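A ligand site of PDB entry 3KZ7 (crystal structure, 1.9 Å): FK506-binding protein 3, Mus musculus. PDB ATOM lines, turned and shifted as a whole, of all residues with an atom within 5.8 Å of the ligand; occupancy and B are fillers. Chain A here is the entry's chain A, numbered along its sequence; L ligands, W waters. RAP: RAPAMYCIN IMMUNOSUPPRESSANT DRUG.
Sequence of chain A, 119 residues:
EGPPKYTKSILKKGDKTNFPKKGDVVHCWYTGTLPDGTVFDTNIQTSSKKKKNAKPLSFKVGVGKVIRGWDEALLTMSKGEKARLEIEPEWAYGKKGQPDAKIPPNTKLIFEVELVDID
An oxygen (O3) of the ligand is in hydrogen-bond range of the side-chain hydroxyl of Tyr 93.
The side-chain carboxylate of Asp 41 sits at hydrogen-bond distance from an oxygen (O6) of the ligand, at 2.6 Å.
O10 of the ligand is in hydrogen-bond range of O of Lys 65 (2.8 Å).
The side-chain amino group (NZ) of Lys 65 sits at hydrogen-bond distance from an oxygen (O8) of the ligand, at 3.2 Å.
The backbone carbonyl oxygen of Gly 64 is in hydrogen-bond range of an oxygen (O13) of the ligand (2.8 Å).
An oxygen (O2) of the ligand lies within hydrogen-bond range of the backbone NH (N) of Ile 67 (3.0 Å).
OD2 of Asp 41 lies within hydrogen-bond range of OH of Tyr 30, 2.6 Å away.
O of Asp 41 lies within hydrogen-bond range of N of Gly 32 (2.9 Å).
The backbone NH of Phe 40 is in hydrogen-bond range of the backbone carbonyl oxygen of Gly 32, at 2.9 Å.
Tyr 30 touches the ligand.
CE1 of Phe 40 touches O4 of the ligand, 3.6 Å away.
CD2 of Leu 57 touches C5 of the ligand (3.4 Å).
Val 66 touches the ligand.
Trp 70 touches the ligand.
CG1 of Ile 103 touches C43 of the ligand, 3.95 Å away.
Phe 111 touches the ligand.
Hydrophobic or aromatic side chains within 4 Å of the ligand: Tyr 30, Phe 40, Leu 57, Val 66, Ile 67, Trp 70, Tyr 93, Ile 103 and Phe 111.
Water W1 lies within hydrogen-bond range of the side-chain carboxylate (OD1) of Asp 41 (2.8 Å) and an oxygen (O7) of the ligand (2.9 Å).
Water W2 bridges O of Ala 101 (2.9 Å) and O6 of the ligand (3.0 Å).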
ATOM      1  N   TYR A  30      29.573  -8.958   1.009  1.00  0.00           N
ATOM      2  CA  TYR A  30      29.555  -9.019   2.449  1.00  0.00           C
ATOM      3  C   TYR A  30      29.624 -10.443   3.026  1.00  0.00           C
ATOM      4  O   TYR A  30      29.288 -11.408   2.378  1.00  0.00           O
ATOM      5  CB  TYR A  30      28.328  -8.318   3.013  1.00  0.00           C
ATOM      6  CG  TYR A  30      27.078  -9.086   2.825  1.00  0.00           C
ATOM      7  CD1 TYR A  30      26.380  -9.019   1.649  1.00  0.00           C
ATOM      8  CD2 TYR A  30      26.607  -9.914   3.791  1.00  0.00           C
ATOM      9  CE1 TYR A  30      25.288  -9.710   1.469  1.00  0.00           C
ATOM     10  CE2 TYR A  30      25.497 -10.592   3.632  1.00  0.00           C
ATOM     11  CZ  TYR A  30      24.827 -10.515   2.453  1.00  0.00           C
ATOM     12  OH  TYR A  30      23.714 -11.230   2.300  1.00  0.00           O
ATOM     13  N   GLY A  32      28.570 -11.923   7.000  1.00  0.00           N
ATOM     14  CA  GLY A  32      27.981 -11.674   8.290  1.00  0.00           C
ATOM     15  C   GLY A  32      28.288 -12.800   9.250  1.00  0.00           C
ATOM     16  O   GLY A  32      28.102 -13.937   8.921  1.00  0.00           O
ATOM     17  N   PHE A  40      26.808 -16.448   9.482  1.00  0.00           N
ATOM     18  CA  PHE A  40      25.410 -16.599   9.226  1.00  0.00           C
ATOM     19  C   PHE A  40      24.970 -16.351   7.777  1.00  0.00           C
ATOM     20  O   PHE A  40      23.987 -16.854   7.373  1.00  0.00           O
ATOM     21  CB  PHE A  40      24.541 -15.847  10.246  1.00  0.00           C
ATOM     22  CG  PHE A  40      24.712 -14.356  10.236  1.00  0.00           C
ATOM     23  CD1 PHE A  40      24.020 -13.582   9.349  1.00  0.00           C
ATOM     24  CD2 PHE A  40      25.520 -13.730  11.123  1.00  0.00           C
ATOM     25  CE1 PHE A  40      24.180 -12.247   9.360  1.00  0.00           C
ATOM     26  CE2 PHE A  40      25.662 -12.407  11.116  1.00  0.00           C
ATOM     27  CZ  PHE A  40      24.998 -11.674  10.240  1.00  0.00           C
ATOM     28  N   ASP A  41      25.693 -15.540   7.039  1.00  0.00           N
ATOM     29  CA  ASP A  41      25.396 -15.271   5.665  1.00  0.00           C
ATOM     30  C   ASP A  41      26.596 -14.695   4.938  1.00  0.00           C
ATOM     31  O   ASP A  41      27.412 -14.072   5.523  1.00  0.00           O
ATOM     32  CB  ASP A  41      24.209 -14.316   5.597  1.00  0.00           C
ATOM     33  CG  ASP A  41      23.667 -14.098   4.196  1.00  0.00           C
ATOM     34  OD1 ASP A  41      23.803 -14.949   3.340  1.00  0.00           O
ATOM     35  OD2 ASP A  41      23.100 -13.063   3.972  1.00  0.00           O
ATOM     36  N   LEU A  57      25.153  -7.411  -3.647  1.00  0.00           N
ATOM     37  CA  LEU A  57      23.967  -6.828  -3.099  1.00  0.00           C
ATOM     38  C   LEU A  57      23.858  -5.391  -3.632  1.00  0.00           C
ATOM     39  O   LEU A  57      24.832  -4.698  -3.705  1.00  0.00           O
ATOM     40  CB  LEU A  57      24.059  -6.830  -1.587  1.00  0.00           C
ATOM     41  CG  LEU A  57      22.856  -6.439  -0.771  1.00  0.00           C
ATOM     42  CD1 LEU A  57      21.813  -7.463  -0.811  1.00  0.00           C
ATOM     43  CD2 LEU A  57      23.251  -6.137   0.618  1.00  0.00           C
ATOM     44  N   SER A  58      22.655  -4.976  -4.005  1.00  0.00           N
ATOM     45  CA  SER A  58      22.255  -3.797  -4.552  1.00  0.00           C
ATOM     46  C   SER A  58      21.205  -3.114  -3.794  1.00  0.00           C
ATOM     47  O   SER A  58      20.214  -3.711  -3.532  1.00  0.00           O
ATOM     48  CB  SER A  58      21.818  -3.901  -6.014  1.00  0.00           C
ATOM     49  OG  SER A  58      22.935  -4.109  -6.873  1.00  0.00           O
ATOM     50  N   PHE A  59      21.384  -1.862  -3.403  1.00  0.00           N
ATOM     51  CA  PHE A  59      20.362  -1.151  -2.639  1.00  0.00           C
ATOM     52  C   PHE A  59      20.690   0.297  -2.712  1.00  0.00           C
ATOM     53  O   PHE A  59      21.769   0.753  -2.818  1.00  0.00           O
ATOM     54  CB  PHE A  59      20.211  -1.653  -1.201  1.00  0.00           C
ATOM     55  CG  PHE A  59      21.454  -1.489  -0.360  1.00  0.00           C
ATOM     56  CD1 PHE A  59      22.461  -2.439  -0.392  1.00  0.00           C
ATOM     57  CD2 PHE A  59      21.601  -0.393   0.473  1.00  0.00           C
ATOM     58  CE1 PHE A  59      23.598  -2.287   0.376  1.00  0.00           C
ATOM     59  CE2 PHE A  59      22.738  -0.241   1.240  1.00  0.00           C
ATOM     60  CZ  PHE A  59      23.727  -1.186   1.200  1.00  0.00           C
ATOM     61  N   GLY A  64      16.703   3.452   4.587  1.00  0.00           N
ATOM     62  CA  GLY A  64      16.080   2.408   5.353  1.00  0.00           C
ATOM     63  C   GLY A  64      15.806   1.097   4.670  1.00  0.00           C
ATOM     64  O   GLY A  64      14.989   0.368   5.107  1.00  0.00           O
ATOM     65  N   LYS A  65      16.474   0.847   3.570  1.00  0.00           N
ATOM     66  CA  LYS A  65      16.417  -0.433   2.912  1.00  0.00           C
ATOM     67  C   LYS A  65      17.176  -1.552   3.612  1.00  0.00           C
ATOM     68  O   LYS A  65      16.905  -2.684   3.412  1.00  0.00           O
ATOM     69  CB  LYS A  65      16.784  -0.323   1.448  1.00  0.00           C
ATOM     70  CG  LYS A  65      15.737   0.430   0.684  1.00  0.00           C
ATOM     71  CD  LYS A  65      15.736   0.095  -0.728  1.00  0.00           C
ATOM     72  CE  LYS A  65      14.584   0.773  -1.466  1.00  0.00           C
ATOM     73  NZ  LYS A  65      13.252   0.490  -0.901  1.00  0.00           N
ATOM     74  N   VAL A  66      18.140  -1.161   4.435  1.00  0.00           N
ATOM     75  CA  VAL A  66      19.003  -2.052   5.182  1.00  0.00           C
ATOM     76  C   VAL A  66      19.061  -1.591   6.626  1.00  0.00           C
ATOM     77  O   VAL A  66      18.713  -0.494   6.915  1.00  0.00           O
ATOM     78  CB  VAL A  66      20.412  -2.131   4.634  1.00  0.00           C
ATOM     79  CG1 VAL A  66      20.473  -2.805   3.330  1.00  0.00           C
ATOM     80  CG2 VAL A  66      21.035  -0.804   4.589  1.00  0.00           C
ATOM     81  N   ILE A  67      19.584  -2.423   7.493  1.00  0.00           N
ATOM     82  CA  ILE A  67      19.675  -2.103   8.902  1.00  0.00           C
ATOM     83  C   ILE A  67      20.507  -0.826   9.107  1.00  0.00           C
ATOM     84  O   ILE A  67      21.303  -0.465   8.316  1.00  0.00           O
ATOM     85  CB  ILE A  67      20.237  -3.288   9.728  1.00  0.00           C
ATOM     86  CG1 ILE A  67      21.616  -3.710   9.239  1.00  0.00           C
ATOM     87  CG2 ILE A  67      19.280  -4.485   9.687  1.00  0.00           C
ATOM     88  CD1 ILE A  67      22.240  -4.729  10.042  1.00  0.00           C
ATOM     89  N   TRP A  70      24.368  -0.564   8.641  1.00  0.00           N
ATOM     90  CA  TRP A  70      24.805  -0.572   7.268  1.00  0.00           C
ATOM     91  C   TRP A  70      24.547   0.780   6.587  1.00  0.00           C
ATOM     92  O   TRP A  70      25.363   1.291   5.919  1.00  0.00           O
ATOM     93  CB  TRP A  70      24.136  -1.675   6.484  1.00  0.00           C
ATOM     94  CG  TRP A  70      24.818  -2.993   6.415  1.00  0.00           C
ATOM     95  CD1 TRP A  70      25.049  -3.837   7.423  1.00  0.00           C
ATOM     96  CD2 TRP A  70      25.296  -3.619   5.258  1.00  0.00           C
ATOM     97  NE1 TRP A  70      25.655  -4.964   6.990  1.00  0.00           N
ATOM     98  CE2 TRP A  70      25.809  -4.861   5.630  1.00  0.00           C
ATOM     99  CE3 TRP A  70      25.345  -3.261   3.916  1.00  0.00           C
ATOM    100  CZ2 TRP A  70      26.366  -5.725   4.729  1.00  0.00           C
ATOM    101  CZ3 TRP A  70      25.893  -4.123   3.035  1.00  0.00           C
ATOM    102  CH2 TRP A  70      26.392  -5.350   3.444  1.00  0.00           C
ATOM    103  N   TYR A  93      18.753  -5.703  14.234  1.00  0.00           N
ATOM    104  CA  TYR A  93      17.408  -6.268  14.274  1.00  0.00           C
ATOM    105  C   TYR A  93      16.715  -6.137  15.633  1.00  0.00           C
ATOM    106  O   TYR A  93      15.719  -6.746  15.898  1.00  0.00           O
ATOM    107  CB  TYR A  93      17.372  -7.708  13.730  1.00  0.00           C
ATOM    108  CG  TYR A  93      17.818  -7.813  12.304  1.00  0.00           C
ATOM    109  CD1 TYR A  93      16.965  -7.521  11.277  1.00  0.00           C
ATOM    110  CD2 TYR A  93      19.095  -8.147  11.984  1.00  0.00           C
ATOM    111  CE1 TYR A  93      17.370  -7.572   9.991  1.00  0.00           C
ATOM    112  CE2 TYR A  93      19.505  -8.186  10.719  1.00  0.00           C
ATOM    113  CZ  TYR A  93      18.638  -7.906   9.716  1.00  0.00           C
ATOM    114  OH  TYR A  93      19.016  -7.949   8.442  1.00  0.00           O
ATOM    115  N   ALA A 101      15.342 -15.486  10.357  1.00  0.00           N
ATOM    116  CA  ALA A 101      16.494 -15.184   9.534  1.00  0.00           C
ATOM    117  C   ALA A 101      17.815 -15.593  10.189  1.00  0.00           C
ATOM    118  O   ALA A 101      18.865 -15.191   9.731  1.00  0.00           O
ATOM    119  CB  ALA A 101      16.505 -13.755   9.201  1.00  0.00           C
ATOM    120  N   ILE A 103      18.987 -14.689  13.175  1.00  0.00           N
ATOM    121  CA  ILE A 103      19.629 -13.701  13.989  1.00  0.00           C
ATOM    122  C   ILE A 103      19.082 -13.772  15.395  1.00  0.00           C
ATOM    123  O   ILE A 103      17.968 -13.441  15.638  1.00  0.00           O
ATOM    124  CB  ILE A 103      19.411 -12.306  13.418  1.00  0.00           C
ATOM    125  CG1 ILE A 103      19.792 -12.255  11.936  1.00  0.00           C
ATOM    126  CG2 ILE A 103      20.161 -11.320  14.223  1.00  0.00           C
ATOM    127  CD1 ILE A 103      21.163 -12.516  11.684  1.00  0.00           C
ATOM    128  N   LEU A 109      26.172  -7.904  15.603  1.00  0.00           N
ATOM    129  CA  LEU A 109      26.445  -8.552  14.356  1.00  0.00           C
ATOM    130  C   LEU A 109      27.732  -7.996  13.791  1.00  0.00           C
ATOM    131  O   LEU A 109      27.955  -6.834  13.848  1.00  0.00           O
ATOM    132  CB  LEU A 109      25.307  -8.334  13.394  1.00  0.00           C
ATOM    133  CG  LEU A 109      23.964  -8.933  13.764  1.00  0.00           C
ATOM    134  CD1 LEU A 109      22.937  -8.627  12.749  1.00  0.00           C
ATOM    135  CD2 LEU A 109      24.062 -10.362  14.063  1.00  0.00           C
ATOM    136  N   PHE A 111      29.892  -7.672  10.375  1.00  0.00           N
ATOM    137  CA  PHE A 111      29.944  -7.769   8.932  1.00  0.00           C
ATOM    138  C   PHE A 111      31.282  -7.265   8.374  1.00  0.00           C
ATOM    139  O   PHE A 111      31.819  -6.316   8.835  1.00  0.00           O
ATOM    140  CB  PHE A 111      28.849  -6.974   8.221  1.00  0.00           C
ATOM    141  CG  PHE A 111      27.447  -7.403   8.507  1.00  0.00           C
ATOM    142  CD1 PHE A 111      26.748  -8.195   7.648  1.00  0.00           C
ATOM    143  CD2 PHE A 111      26.799  -6.938   9.581  1.00  0.00           C
ATOM    144  CE1 PHE A 111      25.482  -8.510   7.895  1.00  0.00           C
ATOM    145  CE2 PHE A 111      25.518  -7.272   9.823  1.00  0.00           C
ATOM    146  CZ  PHE A 111      24.872  -8.061   8.973  1.00  0.00           C
HETATM  147  C1  RAP L   1      20.044  -6.144   5.857  1.00  0.00           C
HETATM  148  O1  RAP L   1      19.181  -7.040   5.151  1.00  0.00           O
HETATM  149  O2  RAP L   1      19.664  -5.051   6.137  1.00  0.00           O
HETATM  150  C2  RAP L   1      21.397  -6.652   6.243  1.00  0.00           C
HETATM  151  C3  RAP L   1      22.476  -5.742   5.689  1.00  0.00           C
HETATM  152  C4  RAP L   1      22.664  -5.837   4.205  1.00  0.00           C
HETATM  153  C5  RAP L   1      22.934  -7.256   3.828  1.00  0.00           C
HETATM  154  C6  RAP L   1      21.986  -8.249   4.464  1.00  0.00           C
HETATM  155  N7  RAP L   1      21.694  -8.026   5.840  1.00  0.00           N
HETATM  156  C8  RAP L   1      21.629  -8.998   6.714  1.00  0.00           C
HETATM  157  O3  RAP L   1      21.332  -8.814   7.838  1.00  0.00           O
HETATM  158  C9  RAP L   1      21.932 -10.349   6.288  1.00  0.00           C
HETATM  159  O4  RAP L   1      23.033 -10.712   6.263  1.00  0.00           O
HETATM  160  C10 RAP L   1      20.896 -11.320   5.793  1.00  0.00           C
HETATM  161  O5  RAP L   1      20.624 -10.930   4.467  1.00  0.00           O
HETATM  162  O6  RAP L   1      21.437 -12.613   5.864  1.00  0.00           O
HETATM  163  C11 RAP L   1      19.604 -11.201   6.601  1.00  0.00           C
HETATM  164  C12 RAP L   1      18.476 -11.955   5.910  1.00  0.00           C
HETATM  165  C13 RAP L   1      18.320 -11.498   4.484  1.00  0.00           C
HETATM  166  C14 RAP L   1      19.632 -11.631   3.746  1.00  0.00           C
HETATM  167  C15 RAP L   1      19.566 -11.015   2.351  1.00  0.00           C
HETATM  168  C16 RAP L   1      18.828 -11.804   1.291  1.00  0.00           C
HETATM  169  O7  RAP L   1      19.616 -12.918   0.965  1.00  0.00           O
HETATM  170  C17 RAP L   1      18.600 -10.910   0.118  1.00  0.00           C
HETATM  171  C18 RAP L   1      17.387 -10.487  -0.182  1.00  0.00           C
HETATM  172  C19 RAP L   1      17.035  -9.606  -1.274  1.00  0.00           C
HETATM  173  C20 RAP L   1      15.811  -9.136  -1.379  1.00  0.00           C
HETATM  174  C21 RAP L   1      15.338  -8.220  -2.391  1.00  0.00           C
HETATM  175  C22 RAP L   1      14.175  -7.617  -2.279  1.00  0.00           C
HETATM  176  C23 RAP L   1      13.641  -6.591  -3.238  1.00  0.00           C
HETATM  177  C24 RAP L   1      13.125  -5.436  -2.428  1.00  0.00           C
HETATM  178  C25 RAP L   1      14.168  -4.790  -1.561  1.00  0.00           C
HETATM  179  C26 RAP L   1      13.526  -3.841  -0.622  1.00  0.00           C
HETATM  180  O8  RAP L   1      13.406  -2.712  -0.925  1.00  0.00           O
HETATM  181  C27 RAP L   1      13.071  -4.355   0.695  1.00  0.00           C
HETATM  182  O9  RAP L   1      11.952  -3.652   1.112  1.00  0.00           O
HETATM  183  C28 RAP L   1      14.229  -4.273   1.685  1.00  0.00           C
HETATM  184  O10 RAP L   1      14.956  -3.102   1.517  1.00  0.00           O
HETATM  185  C29 RAP L   1      15.099  -5.453   1.457  1.00  0.00           C
HETATM  186  C30 RAP L   1      16.412  -5.334   1.325  1.00  0.00           C
HETATM  187  C31 RAP L   1      17.328  -6.490   1.112  1.00  0.00           C
HETATM  188  C32 RAP L   1      18.198  -6.653   2.326  1.00  0.00           C
HETATM  189  O11 RAP L   1      19.321  -6.299   2.326  1.00  0.00           O
HETATM  190  C33 RAP L   1      17.589  -7.309   3.541  1.00  0.00           C
HETATM  191  C34 RAP L   1      17.891  -6.566   4.827  1.00  0.00           C
HETATM  192  C35 RAP L   1      16.905  -6.880   5.942  1.00  0.00           C
HETATM  193  C36 RAP L   1      15.541  -6.263   5.741  1.00  0.00           C
HETATM  194  C37 RAP L   1      15.457  -4.758   5.908  1.00  0.00           C
HETATM  195  C38 RAP L   1      14.022  -4.306   5.750  1.00  0.00           C
HETATM  196  C39 RAP L   1      13.907  -2.813   5.878  1.00  0.00           C
HETATM  197  O12 RAP L   1      12.569  -2.441   5.756  1.00  0.00           O
HETATM  198  C40 RAP L   1      14.399  -2.407   7.252  1.00  0.00           C
HETATM  199  O13 RAP L   1      14.264  -1.034   7.463  1.00  0.00           O
HETATM  200  C41 RAP L   1      15.841  -2.783   7.348  1.00  0.00           C
HETATM  201  C42 RAP L   1      15.982  -4.284   7.232  1.00  0.00           C
HETATM  202  C43 RAP L   1      19.767 -11.619   8.037  1.00  0.00           C
HETATM  203  C44 RAP L   1      19.754 -10.521  -0.702  1.00  0.00           C
HETATM  204  C45 RAP L   1      12.495  -7.093  -4.089  1.00  0.00           C
HETATM  205  C46 RAP L   1      15.203  -4.102  -2.402  1.00  0.00           C
HETATM  206  C47 RAP L   1      14.472  -6.791   1.481  1.00  0.00           C
HETATM  207  C48 RAP L   1      18.238  -6.204  -0.051  1.00  0.00           C
HETATM  208  C49 RAP L   1      16.773  -8.374   6.129  1.00  0.00           C
HETATM  209  C50 RAP L   1      18.968 -14.021   0.399  1.00  0.00           C
HETATM  210  C51 RAP L   1      12.199  -2.314   1.064  1.00  0.00           C
HETATM  211  C52 RAP L   1      12.259  -2.000   4.468  1.00  0.00           C
HETATM  212  O   HOH W   1      21.594 -14.865   1.700  1.00  0.00           O
HETATM  213  O   HOH W   2      20.323 -15.026   7.250  1.00  0.00           O
HETATM  214  O   HOH W   3      10.538  -2.756   8.110  1.00  0.00           O
